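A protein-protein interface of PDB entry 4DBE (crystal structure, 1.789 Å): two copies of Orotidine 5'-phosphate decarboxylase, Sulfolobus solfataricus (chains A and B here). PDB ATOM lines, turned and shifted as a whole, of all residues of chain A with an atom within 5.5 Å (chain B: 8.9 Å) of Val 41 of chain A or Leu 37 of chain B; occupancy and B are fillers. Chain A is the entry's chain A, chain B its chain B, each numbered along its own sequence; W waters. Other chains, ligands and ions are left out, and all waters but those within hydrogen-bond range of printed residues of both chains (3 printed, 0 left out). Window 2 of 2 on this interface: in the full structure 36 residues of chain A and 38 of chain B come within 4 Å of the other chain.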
ATOM      1  N   LEU A  33     -26.778   6.791   1.851  1.00  0.00           N
ATOM      2  CA  LEU A  33     -25.449   7.159   1.369  1.00  0.00           C
ATOM      3  C   LEU A  33     -24.409   7.340   2.494  1.00  0.00           C
ATOM      4  O   LEU A  33     -23.279   6.896   2.361  1.00  0.00           O
ATOM      5  CB  LEU A  33     -25.525   8.405   0.469  1.00  0.00           C
ATOM      6  CG  LEU A  33     -24.222   8.791  -0.236  1.00  0.00           C
ATOM      7  CD1 LEU A  33     -23.586   7.563  -0.956  1.00  0.00           C
ATOM      8  CD2 LEU A  33     -24.461   9.932  -1.209  1.00  0.00           C
ATOM      9  N   VAL A  36     -23.011   3.900   3.317  1.00  0.00           N
ATOM     10  CA  VAL A  36     -22.153   3.308   2.284  1.00  0.00           C
ATOM     11  C   VAL A  36     -20.815   4.037   2.195  1.00  0.00           C
ATOM     12  O   VAL A  36     -19.766   3.406   1.997  1.00  0.00           O
ATOM     13  CB  VAL A  36     -22.849   3.253   0.901  1.00  0.00           C
ATOM     14  CG1 VAL A  36     -21.895   2.699  -0.153  1.00  0.00           C
ATOM     15  CG2 VAL A  36     -24.108   2.390   0.970  1.00  0.00           C
ATOM     16  N   LEU A  39     -18.789   2.650   5.316  1.00  0.00           N
ATOM     17  CA  LEU A  39     -18.347   1.261   5.256  1.00  0.00           C
ATOM     18  C   LEU A  39     -17.660   0.873   3.952  1.00  0.00           C
ATOM     19  O   LEU A  39     -16.830  -0.041   3.932  1.00  0.00           O
ATOM     20  CB  LEU A  39     -19.506   0.303   5.504  1.00  0.00           C
ATOM     21  CG  LEU A  39     -20.274   0.465   6.807  1.00  0.00           C
ATOM     22  CD1 LEU A  39     -21.261  -0.686   6.983  1.00  0.00           C
ATOM     23  CD2 LEU A  39     -19.298   0.532   7.958  1.00  0.00           C
ATOM     24  N   GLY A  40     -18.008   1.561   2.868  1.00  0.00           N
ATOM     25  CA  GLY A  40     -17.613   1.131   1.537  1.00  0.00           C
ATOM     26  C   GLY A  40     -18.644   0.153   1.022  1.00  0.00           C
ATOM     27  O   GLY A  40     -19.386  -0.423   1.814  1.00  0.00           O
ATOM     28  N   VAL A  41     -18.672  -0.050  -0.293  1.00  0.00           N
ATOM     29  CA  VAL A  41     -19.643  -0.946  -0.924  1.00  0.00           C
ATOM     30  C   VAL A  41     -19.408  -2.389  -0.486  1.00  0.00           C
ATOM     31  O   VAL A  41     -20.339  -3.096  -0.115  1.00  0.00           O
ATOM     32  CB  VAL A  41     -19.597  -0.824  -2.461  1.00  0.00           C
ATOM     33  CG1 VAL A  41     -20.425  -1.939  -3.131  1.00  0.00           C
ATOM     34  CG2 VAL A  41     -20.088   0.565  -2.890  1.00  0.00           C
ATOM     35  N   ASP A  42     -18.155  -2.819  -0.511  1.00  0.00           N
ATOM     36  CA  ASP A  42     -17.827  -4.202  -0.147  1.00  0.00           C
ATOM     37  C   ASP A  42     -18.295  -4.583   1.255  1.00  0.00           C
ATOM     38  O   ASP A  42     -18.910  -5.627   1.446  1.00  0.00           O
ATOM     39  CB  ASP A  42     -16.325  -4.473  -0.312  1.00  0.00           C
ATOM     40  CG  ASP A  42     -15.881  -4.436  -1.769  1.00  0.00           C
ATOM     41  OD1 ASP A  42     -16.744  -4.599  -2.667  1.00  0.00           O
ATOM     42  OD2 ASP A  42     -14.665  -4.244  -2.020  1.00  0.00           O
ATOM     43  N   LYS A  43     -18.014  -3.739   2.238  1.00  0.00           N
ATOM     44  CA  LYS A  43     -18.419  -4.041   3.594  1.00  0.00           C
ATOM     45  C   LYS A  43     -19.925  -3.849   3.789  1.00  0.00           C
ATOM     46  O   LYS A  43     -20.538  -4.536   4.602  1.00  0.00           O
ATOM     47  CB  LYS A  43     -17.597  -3.233   4.595  1.00  0.00           C
ATOM     48  CG  LYS A  43     -16.102  -3.630   4.604  1.00  0.00           C
ATOM     49  CD  LYS A  43     -15.945  -5.068   5.106  1.00  0.00           C
ATOM     50  CE  LYS A  43     -14.486  -5.536   5.123  1.00  0.00           C
ATOM     51  NZ  LYS A  43     -14.371  -6.846   5.828  1.00  0.00           N
ATOM     52  N   THR A  44     -20.527  -2.927   3.040  1.00  0.00           N
ATOM     53  CA  THR A  44     -21.984  -2.797   3.096  1.00  0.00           C
ATOM     54  C   THR A  44     -22.651  -4.097   2.620  1.00  0.00           C
ATOM     55  O   THR A  44     -23.575  -4.614   3.255  1.00  0.00           O
ATOM     56  CB  THR A  44     -22.481  -1.607   2.251  1.00  0.00           C
ATOM     57  OG1 THR A  44     -21.890  -0.398   2.747  1.00  0.00           O
ATOM     58  CG2 THR A  44     -24.010  -1.496   2.332  1.00  0.00           C
ATOM     59  N   ARG A  45     -22.171  -4.622   1.496  1.00  0.00           N
ATOM     60  CA  ARG A  45     -22.671  -5.880   0.955  1.00  0.00           C
ATOM     61  C   ARG A  45     -22.477  -7.022   1.966  1.00  0.00           C
ATOM     62  O   ARG A  45     -23.381  -7.824   2.206  1.00  0.00           O
ATOM     63  CB  ARG A  45     -21.937  -6.198  -0.357  1.00  0.00           C
ATOM     64  CG  ARG A  45     -22.357  -7.491  -1.034  1.00  0.00           C
ATOM     65  CD  ARG A  45     -21.483  -7.799  -2.256  1.00  0.00           C
ATOM     66  NE  ARG A  45     -21.732  -6.895  -3.378  1.00  0.00           N
ATOM     67  CZ  ARG A  45     -22.711  -7.057  -4.270  1.00  0.00           C
ATOM     68  NH1 ARG A  45     -23.551  -8.083  -4.169  1.00  0.00           N
ATOM     69  NH2 ARG A  45     -22.860  -6.188  -5.266  1.00  0.00           N
ATOM     70  N   GLU A  46     -21.292  -7.093   2.560  1.00  0.00           N
ATOM     71  CA  GLU A  46     -21.008  -8.146   3.532  1.00  0.00           C
ATOM     72  C   GLU A  46     -21.972  -8.045   4.710  1.00  0.00           C
ATOM     73  O   GLU A  46     -22.567  -9.042   5.126  1.00  0.00           O
ATOM     74  CB  GLU A  46     -19.555  -8.088   4.003  1.00  0.00           C
ATOM     75  CG  GLU A  46     -19.254  -9.092   5.100  1.00  0.00           C
ATOM     76  CD  GLU A  46     -17.813  -9.032   5.575  1.00  0.00           C
ATOM     77  OE1 GLU A  46     -16.973  -8.443   4.867  1.00  0.00           O
ATOM     78  OE2 GLU A  46     -17.529  -9.576   6.657  1.00  0.00           O
ATOM     79  N   PHE A  60     -29.844   6.355  -2.591  1.00  0.00           N
ATOM     80  CA  PHE A  60     -28.928   7.458  -2.874  1.00  0.00           C
ATOM     81  C   PHE A  60     -29.670   8.644  -3.522  1.00  0.00           C
ATOM     82  O   PHE A  60     -29.045   9.550  -4.077  1.00  0.00           O
ATOM     83  CB  PHE A  60     -27.753   7.006  -3.752  1.00  0.00           C
ATOM     84  CG  PHE A  60     -26.838   5.978  -3.096  1.00  0.00           C
ATOM     85  CD1 PHE A  60     -27.015   5.591  -1.777  1.00  0.00           C
ATOM     86  CD2 PHE A  60     -25.802   5.409  -3.816  1.00  0.00           C
ATOM     87  CE1 PHE A  60     -26.176   4.643  -1.188  1.00  0.00           C
ATOM     88  CE2 PHE A  60     -24.949   4.459  -3.232  1.00  0.00           C
ATOM     89  CZ  PHE A  60     -25.135   4.081  -1.921  1.00  0.00           C
ATOM     90  N   ILE A  72     -24.350   4.162 -11.198  1.00  0.00           N
ATOM     91  CA  ILE A  72     -24.448   4.024  -9.758  1.00  0.00           C
ATOM     92  C   ILE A  72     -25.089   2.697  -9.373  1.00  0.00           C
ATOM     93  O   ILE A  72     -24.548   1.956  -8.561  1.00  0.00           O
ATOM     94  CB  ILE A  72     -25.262   5.190  -9.143  1.00  0.00           C
ATOM     95  CG1 ILE A  72     -24.479   6.502  -9.285  1.00  0.00           C
ATOM     96  CG2 ILE A  72     -25.632   4.887  -7.701  1.00  0.00           C
ATOM     97  CD1 ILE A  72     -25.312   7.743  -9.054  1.00  0.00           C
ATOM     98  N   ARG A  75     -23.411  -0.807  -9.450  1.00  0.00           N
ATOM     99  CA  ARG A  75     -22.386  -1.047  -8.438  1.00  0.00           C
ATOM    100  C   ARG A  75     -22.979  -1.569  -7.130  1.00  0.00           C
ATOM    101  O   ARG A  75     -22.246  -1.864  -6.175  1.00  0.00           O
ATOM    102  CB  ARG A  75     -21.599   0.242  -8.190  1.00  0.00           C
ATOM    103  CG  ARG A  75     -20.639   0.574  -9.310  1.00  0.00           C
ATOM    104  CD  ARG A  75     -20.280   2.044  -9.366  1.00  0.00           C
ATOM    105  NE  ARG A  75     -19.052   2.226 -10.133  1.00  0.00           N
ATOM    106  CZ  ARG A  75     -18.994   2.235 -11.463  1.00  0.00           C
ATOM    107  NH1 ARG A  75     -20.102   2.102 -12.173  1.00  0.00           N
ATOM    108  NH2 ARG A  75     -17.830   2.390 -12.081  1.00  0.00           N
ATOM    109  N   LEU A  76     -24.305  -1.695  -7.097  1.00  0.00           N
ATOM    110  CA  LEU A  76     -25.028  -1.988  -5.861  1.00  0.00           C
ATOM    111  C   LEU A  76     -26.005  -3.154  -6.020  1.00  0.00           C
ATOM    112  O   LEU A  76     -27.142  -3.086  -5.543  1.00  0.00           O
ATOM    113  CB  LEU A  76     -25.796  -0.730  -5.406  1.00  0.00           C
ATOM    114  CG  LEU A  76     -24.936   0.537  -5.411  1.00  0.00           C
ATOM    115  CD1 LEU A  76     -25.783   1.807  -5.383  1.00  0.00           C
ATOM    116  CD2 LEU A  76     -23.925   0.509  -4.259  1.00  0.00           C
ATOM    117  N   PHE A  78     -26.545  -5.805  -4.624  1.00  0.00           N
ATOM    118  CA  PHE A  78     -27.078  -6.465  -3.434  1.00  0.00           C
ATOM    119  C   PHE A  78     -28.476  -5.966  -3.042  1.00  0.00           C
ATOM    120  O   PHE A  78     -29.171  -6.605  -2.246  1.00  0.00           O
ATOM    121  CB  PHE A  78     -26.127  -6.296  -2.252  1.00  0.00           C
ATOM    122  CG  PHE A  78     -25.813  -4.874  -1.931  1.00  0.00           C
ATOM    123  CD1 PHE A  78     -26.639  -4.139  -1.092  1.00  0.00           C
ATOM    124  CD2 PHE A  78     -24.685  -4.270  -2.457  1.00  0.00           C
ATOM    125  CE1 PHE A  78     -26.339  -2.823  -0.790  1.00  0.00           C
ATOM    126  CE2 PHE A  78     -24.381  -2.952  -2.159  1.00  0.00           C
ATOM    127  CZ  PHE A  78     -25.205  -2.229  -1.330  1.00  0.00           C
ATOM    128  N   MET B  10     -14.934  13.417 -13.181  1.00  0.00           N
ATOM    129  CA  MET B  10     -14.375  12.109 -12.858  1.00  0.00           C
ATOM    130  C   MET B  10     -15.453  11.186 -12.357  1.00  0.00           C
ATOM    131  O   MET B  10     -15.669  11.092 -11.144  1.00  0.00           O
ATOM    132  CB  MET B  10     -13.320  12.209 -11.743  1.00  0.00           C
ATOM    133  CG  MET B  10     -11.945  12.630 -12.152  1.00  0.00           C
ATOM    134  SD  MET B  10     -10.807  12.052 -10.867  1.00  0.00           S
ATOM    135  CE  MET B  10     -10.623  10.352 -11.376  1.00  0.00           C
ATOM    136  N   ASP B  11     -16.128  10.500 -13.278  1.00  0.00           N
ATOM    137  CA  ASP B  11     -17.182   9.561 -12.906  1.00  0.00           C
ATOM    138  C   ASP B  11     -16.727   8.121 -12.999  1.00  0.00           C
ATOM    139  O   ASP B  11     -17.499   7.210 -12.708  1.00  0.00           O
ATOM    140  CB  ASP B  11     -18.420   9.776 -13.775  1.00  0.00           C
ATOM    141  CG  ASP B  11     -19.053  11.108 -13.534  1.00  0.00           C
ATOM    142  OD1 ASP B  11     -19.237  11.448 -12.348  1.00  0.00           O
ATOM    143  OD2 ASP B  11     -19.331  11.828 -14.521  1.00  0.00           O
ATOM    144  N   PRO B  13     -12.630   5.981 -12.446  1.00  0.00           N
ATOM    145  CA  PRO B  13     -11.241   6.235 -12.040  1.00  0.00           C
ATOM    146  C   PRO B  13     -10.327   6.541 -13.223  1.00  0.00           C
ATOM    147  O   PRO B  13     -10.488   5.980 -14.310  1.00  0.00           O
ATOM    148  CB  PRO B  13     -10.816   4.913 -11.387  1.00  0.00           C
ATOM    149  CG  PRO B  13     -12.079   4.227 -11.019  1.00  0.00           C
ATOM    150  CD  PRO B  13     -13.091   4.639 -12.051  1.00  0.00           C
ATOM    151  N   VAL B  31     -15.960  15.358  -8.653  1.00  0.00           N
ATOM    152  CA  VAL B  31     -15.953  13.971  -8.195  1.00  0.00           C
ATOM    153  C   VAL B  31     -17.373  13.395  -8.249  1.00  0.00           C
ATOM    154  O   VAL B  31     -18.277  13.897  -7.587  1.00  0.00           O
ATOM    155  CB  VAL B  31     -15.421  13.864  -6.756  1.00  0.00           C
ATOM    156  CG1 VAL B  31     -15.274  12.412  -6.354  1.00  0.00           C
ATOM    157  CG2 VAL B  31     -14.089  14.590  -6.635  1.00  0.00           C
ATOM    158  N   GLY B  32     -17.563  12.351  -9.052  1.00  0.00           N
ATOM    159  CA  GLY B  32     -18.862  11.710  -9.172  1.00  0.00           C
ATOM    160  C   GLY B  32     -19.029  10.548  -8.203  1.00  0.00           C
ATOM    161  O   GLY B  32     -18.052  10.019  -7.669  1.00  0.00           O
ATOM    162  N   LEU B  33     -20.278  10.154  -7.974  1.00  0.00           N
ATOM    163  CA  LEU B  33     -20.571   9.064  -7.063  1.00  0.00           C
ATOM    164  C   LEU B  33     -20.005   7.709  -7.503  1.00  0.00           C
ATOM    165  O   LEU B  33     -19.548   6.955  -6.668  1.00  0.00           O
ATOM    166  CB  LEU B  33     -22.082   8.976  -6.791  1.00  0.00           C
ATOM    167  CG  LEU B  33     -22.551   8.055  -5.655  1.00  0.00           C
ATOM    168  CD1 LEU B  33     -21.751   8.272  -4.361  1.00  0.00           C
ATOM    169  CD2 LEU B  33     -24.047   8.242  -5.396  1.00  0.00           C
ATOM    170  N   PRO B  34     -20.065   7.374  -8.807  1.00  0.00           N
ATOM    171  CA  PRO B  34     -19.514   6.056  -9.165  1.00  0.00           C
ATOM    172  C   PRO B  34     -18.022   5.930  -8.818  1.00  0.00           C
ATOM    173  O   PRO B  34     -17.567   4.870  -8.369  1.00  0.00           O
ATOM    174  CB  PRO B  34     -19.744   5.975 -10.685  1.00  0.00           C
ATOM    175  CG  PRO B  34     -20.961   6.835 -10.909  1.00  0.00           C
ATOM    176  CD  PRO B  34     -20.783   7.999  -9.934  1.00  0.00           C
ATOM    177  N   LEU B  35     -17.280   7.013  -9.011  1.00  0.00           N
ATOM    178  CA  LEU B  35     -15.873   7.054  -8.618  1.00  0.00           C
ATOM    179  C   LEU B  35     -15.688   6.695  -7.145  1.00  0.00           C
ATOM    180  O   LEU B  35     -14.867   5.843  -6.798  1.00  0.00           O
ATOM    181  CB  LEU B  35     -15.296   8.450  -8.847  1.00  0.00           C
ATOM    182  CG  LEU B  35     -13.798   8.502  -8.501  1.00  0.00           C
ATOM    183  CD1 LEU B  35     -13.001   7.709  -9.524  1.00  0.00           C
ATOM    184  CD2 LEU B  35     -13.281   9.923  -8.414  1.00  0.00           C
ATOM    185  N   VAL B  36     -16.440   7.370  -6.275  1.00  0.00           N
ATOM    186  CA  VAL B  36     -16.267   7.197  -4.832  1.00  0.00           C
ATOM    187  C   VAL B  36     -16.740   5.811  -4.390  1.00  0.00           C
ATOM    188  O   VAL B  36     -16.178   5.212  -3.476  1.00  0.00           O
ATOM    189  CB  VAL B  36     -16.997   8.304  -4.057  1.00  0.00           C
ATOM    190  CG1 VAL B  36     -16.809   8.145  -2.539  1.00  0.00           C
ATOM    191  CG2 VAL B  36     -16.515   9.665  -4.533  1.00  0.00           C
ATOM    192  N   LEU B  37     -17.775   5.292  -5.040  1.00  0.00           N
ATOM    193  CA  LEU B  37     -18.204   3.927  -4.755  1.00  0.00           C
ATOM    194  C   LEU B  37     -17.092   2.940  -5.121  1.00  0.00           C
ATOM    195  O   LEU B  37     -16.866   1.950  -4.415  1.00  0.00           O
ATOM    196  CB  LEU B  37     -19.481   3.581  -5.527  1.00  0.00           C
ATOM    197  CG  LEU B  37     -20.679   4.441  -5.120  1.00  0.00           C
ATOM    198  CD1 LEU B  37     -21.898   4.150  -6.024  1.00  0.00           C
ATOM    199  CD2 LEU B  37     -21.007   4.260  -3.632  1.00  0.00           C
ATOM    200  N   ASP B  38     -16.403   3.213  -6.226  1.00  0.00           N
ATOM    201  CA  ASP B  38     -15.337   2.335  -6.703  1.00  0.00           C
ATOM    202  C   ASP B  38     -14.111   2.382  -5.797  1.00  0.00           C
ATOM    203  O   ASP B  38     -13.598   1.340  -5.369  1.00  0.00           O
ATOM    204  CB  ASP B  38     -14.901   2.713  -8.123  1.00  0.00           C
ATOM    205  CG  ASP B  38     -15.834   2.186  -9.191  1.00  0.00           C
ATOM    206  OD1 ASP B  38     -16.641   1.272  -8.901  1.00  0.00           O
ATOM    207  OD2 ASP B  38     -15.757   2.699 -10.329  1.00  0.00           O
ATOM    208  N   LEU B  39     -13.636   3.592  -5.507  1.00  0.00           N
ATOM    209  CA  LEU B  39     -12.377   3.742  -4.763  1.00  0.00           C
ATOM    210  C   LEU B  39     -12.567   3.752  -3.256  1.00  0.00           C
ATOM    211  O   LEU B  39     -11.651   3.405  -2.514  1.00  0.00           O
ATOM    212  CB  LEU B  39     -11.651   5.023  -5.170  1.00  0.00           C
ATOM    213  CG  LEU B  39     -11.263   5.118  -6.642  1.00  0.00           C
ATOM    214  CD1 LEU B  39     -10.456   6.396  -6.911  1.00  0.00           C
ATOM    215  CD2 LEU B  39     -10.489   3.876  -7.057  1.00  0.00           C
ATOM    216  N   GLY B  40     -13.755   4.154  -2.808  1.00  0.00           N
ATOM    217  CA  GLY B  40     -13.992   4.407  -1.398  1.00  0.00           C
ATOM    218  C   GLY B  40     -13.587   5.834  -1.085  1.00  0.00           C
ATOM    219  O   GLY B  40     -12.826   6.438  -1.837  1.00  0.00           O
ATOM    220  N   VAL B  41     -14.088   6.386   0.011  1.00  0.00           N
ATOM    221  CA  VAL B  41     -13.788   7.784   0.329  1.00  0.00           C
ATOM    222  C   VAL B  41     -12.297   8.009   0.604  1.00  0.00           C
ATOM    223  O   VAL B  41     -11.696   8.986   0.145  1.00  0.00           O
ATOM    224  CB  VAL B  41     -14.601   8.290   1.543  1.00  0.00           C
ATOM    225  CG1 VAL B  41     -14.028   9.611   2.065  1.00  0.00           C
ATOM    226  CG2 VAL B  41     -16.051   8.463   1.178  1.00  0.00           C
ATOM    227  N   THR B  44     -10.246   8.010  -2.491  1.00  0.00           N
ATOM    228  CA  THR B  44     -10.618   9.206  -3.246  1.00  0.00           C
ATOM    229  C   THR B  44      -9.842  10.414  -2.726  1.00  0.00           C
ATOM    230  O   THR B  44      -9.224  11.142  -3.506  1.00  0.00           O
ATOM    231  CB  THR B  44     -12.142   9.458  -3.190  1.00  0.00           C
ATOM    232  OG1 THR B  44     -12.811   8.346  -3.784  1.00  0.00           O
ATOM    233  CG2 THR B  44     -12.515  10.726  -3.947  1.00  0.00           C
ATOM    234  N   PHE B  60     -22.600  14.566  -5.625  1.00  0.00           N
ATOM    235  CA  PHE B  60     -23.515  13.459  -5.371  1.00  0.00           C
ATOM    236  C   PHE B  60     -24.965  13.939  -5.530  1.00  0.00           C
ATOM    237  O   PHE B  60     -25.881  13.344  -4.970  1.00  0.00           O
ATOM    238  CB  PHE B  60     -23.328  12.885  -3.954  1.00  0.00           C
ATOM    239  CG  PHE B  60     -21.944  12.314  -3.680  1.00  0.00           C
ATOM    240  CD1 PHE B  60     -21.060  12.034  -4.715  1.00  0.00           C
ATOM    241  CD2 PHE B  60     -21.550  12.039  -2.372  1.00  0.00           C
ATOM    242  CE1 PHE B  60     -19.806  11.513  -4.456  1.00  0.00           C
ATOM    243  CE2 PHE B  60     -20.294  11.512  -2.094  1.00  0.00           C
ATOM    244  CZ  PHE B  60     -19.417  11.248  -3.137  1.00  0.00           C
ATOM    245  N   LEU B  76     -16.807  14.244   3.165  1.00  0.00           N
ATOM    246  CA  LEU B  76     -15.970  14.588   2.025  1.00  0.00           C
ATOM    247  C   LEU B  76     -15.466  16.031   2.081  1.00  0.00           C
ATOM    248  O   LEU B  76     -15.377  16.713   1.056  1.00  0.00           O
ATOM    249  CB  LEU B  76     -16.765  14.379   0.740  1.00  0.00           C
ATOM    250  CG  LEU B  76     -17.297  12.954   0.538  1.00  0.00           C
ATOM    251  CD1 LEU B  76     -18.803  13.005   0.373  1.00  0.00           C
ATOM    252  CD2 LEU B  76     -16.622  12.329  -0.661  1.00  0.00           C
HETATM  253  O   HOH W   1     -17.038   2.008  -1.780  1.00  0.00           O
HETATM  254  O   HOH W   2     -28.859  12.278  -4.958  1.00  0.00           O
HETATM  255  O   HOH W   3     -26.794  10.579  -5.430  1.00  0.00           O
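Water W1 bridges the backbone carbonyl oxygen (O) of Leu 37 of chain B (2.6 Å) and the backbone NH (N) of Val 41 of chain A (3.0 Å).
Water W3 lies within hydrogen-bond range of the backbone carbonyl oxygen of Phe 60 of chain A and the backbone carbonyl oxygen of Phe 60 of chain B.
Water W2 lies within hydrogen-bond range of O of Phe 60 of chain A (2.9 Å) and O of Phe 60 of chain B (3.2 Å).
NH2 of Arg 75 of chain A lies within salt-bridge range of OD2 of Asp 38 of chain B.
Among the printed residues, pairs that only touch across the chains: Arg 75 of chain A with Pro 34 of chain B (3.5 Å), Phe 60 of chain A with Leu 33 of chain B (3.7 Å), Leu 33 of chain A with Phe 60 of chain B (3.8 Å), Val 41 of chain A with Leu 37 of chain B (3.8 Å), Ile 72 of chain A with Pro 34 of chain B (3.9 Å), Ile 72 of chain A with Leu 33 of chain B (3.9 Å), Val 36 of chain A with Leu 37 of chain B (3.9 Å), Leu 33 of chain A with Leu 33 of chain B (3.9 Å) and Phe 60 of chain A with Leu 37 of chain B (3.97 Å).
Printed residues of chain B within 4 Å of Phe 60 of chain A: Leu 33 and Leu 37.
Of the printed residues of chain A, Pro 34 of chain B touches Ile 72 (3.9 Å) and Arg 75 (3.5 Å).
Printed residues of chain B that touch a printed residue of chain A: Leu 33, Pro 34, Leu 37, Asp 38 and Phe 60.
Of the 15 printed residues of chain A, 6 touch a printed residue of chain B.
Hydrophobic or aromatic side chains of chain A within 4 Å of the printed part of chain B: Leu 33, Val 36, Val 41, Phe 60 and Ile 72.
Leu 33 of chain B touches its own counterpart, Leu 33 of chain A.
Leu 33 of chain A touches Phe 60 of chain B, and with the chains exchanged Phe 60 of chain A touches Leu 33 of chain B.
Positions printed for both chains: 33, 36, 39, 40, 41, 44, 60 and 76.
Of the 10 pairs that touch across the chains among the printed residues, 3 have their exchanged pair printed and touching as well.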
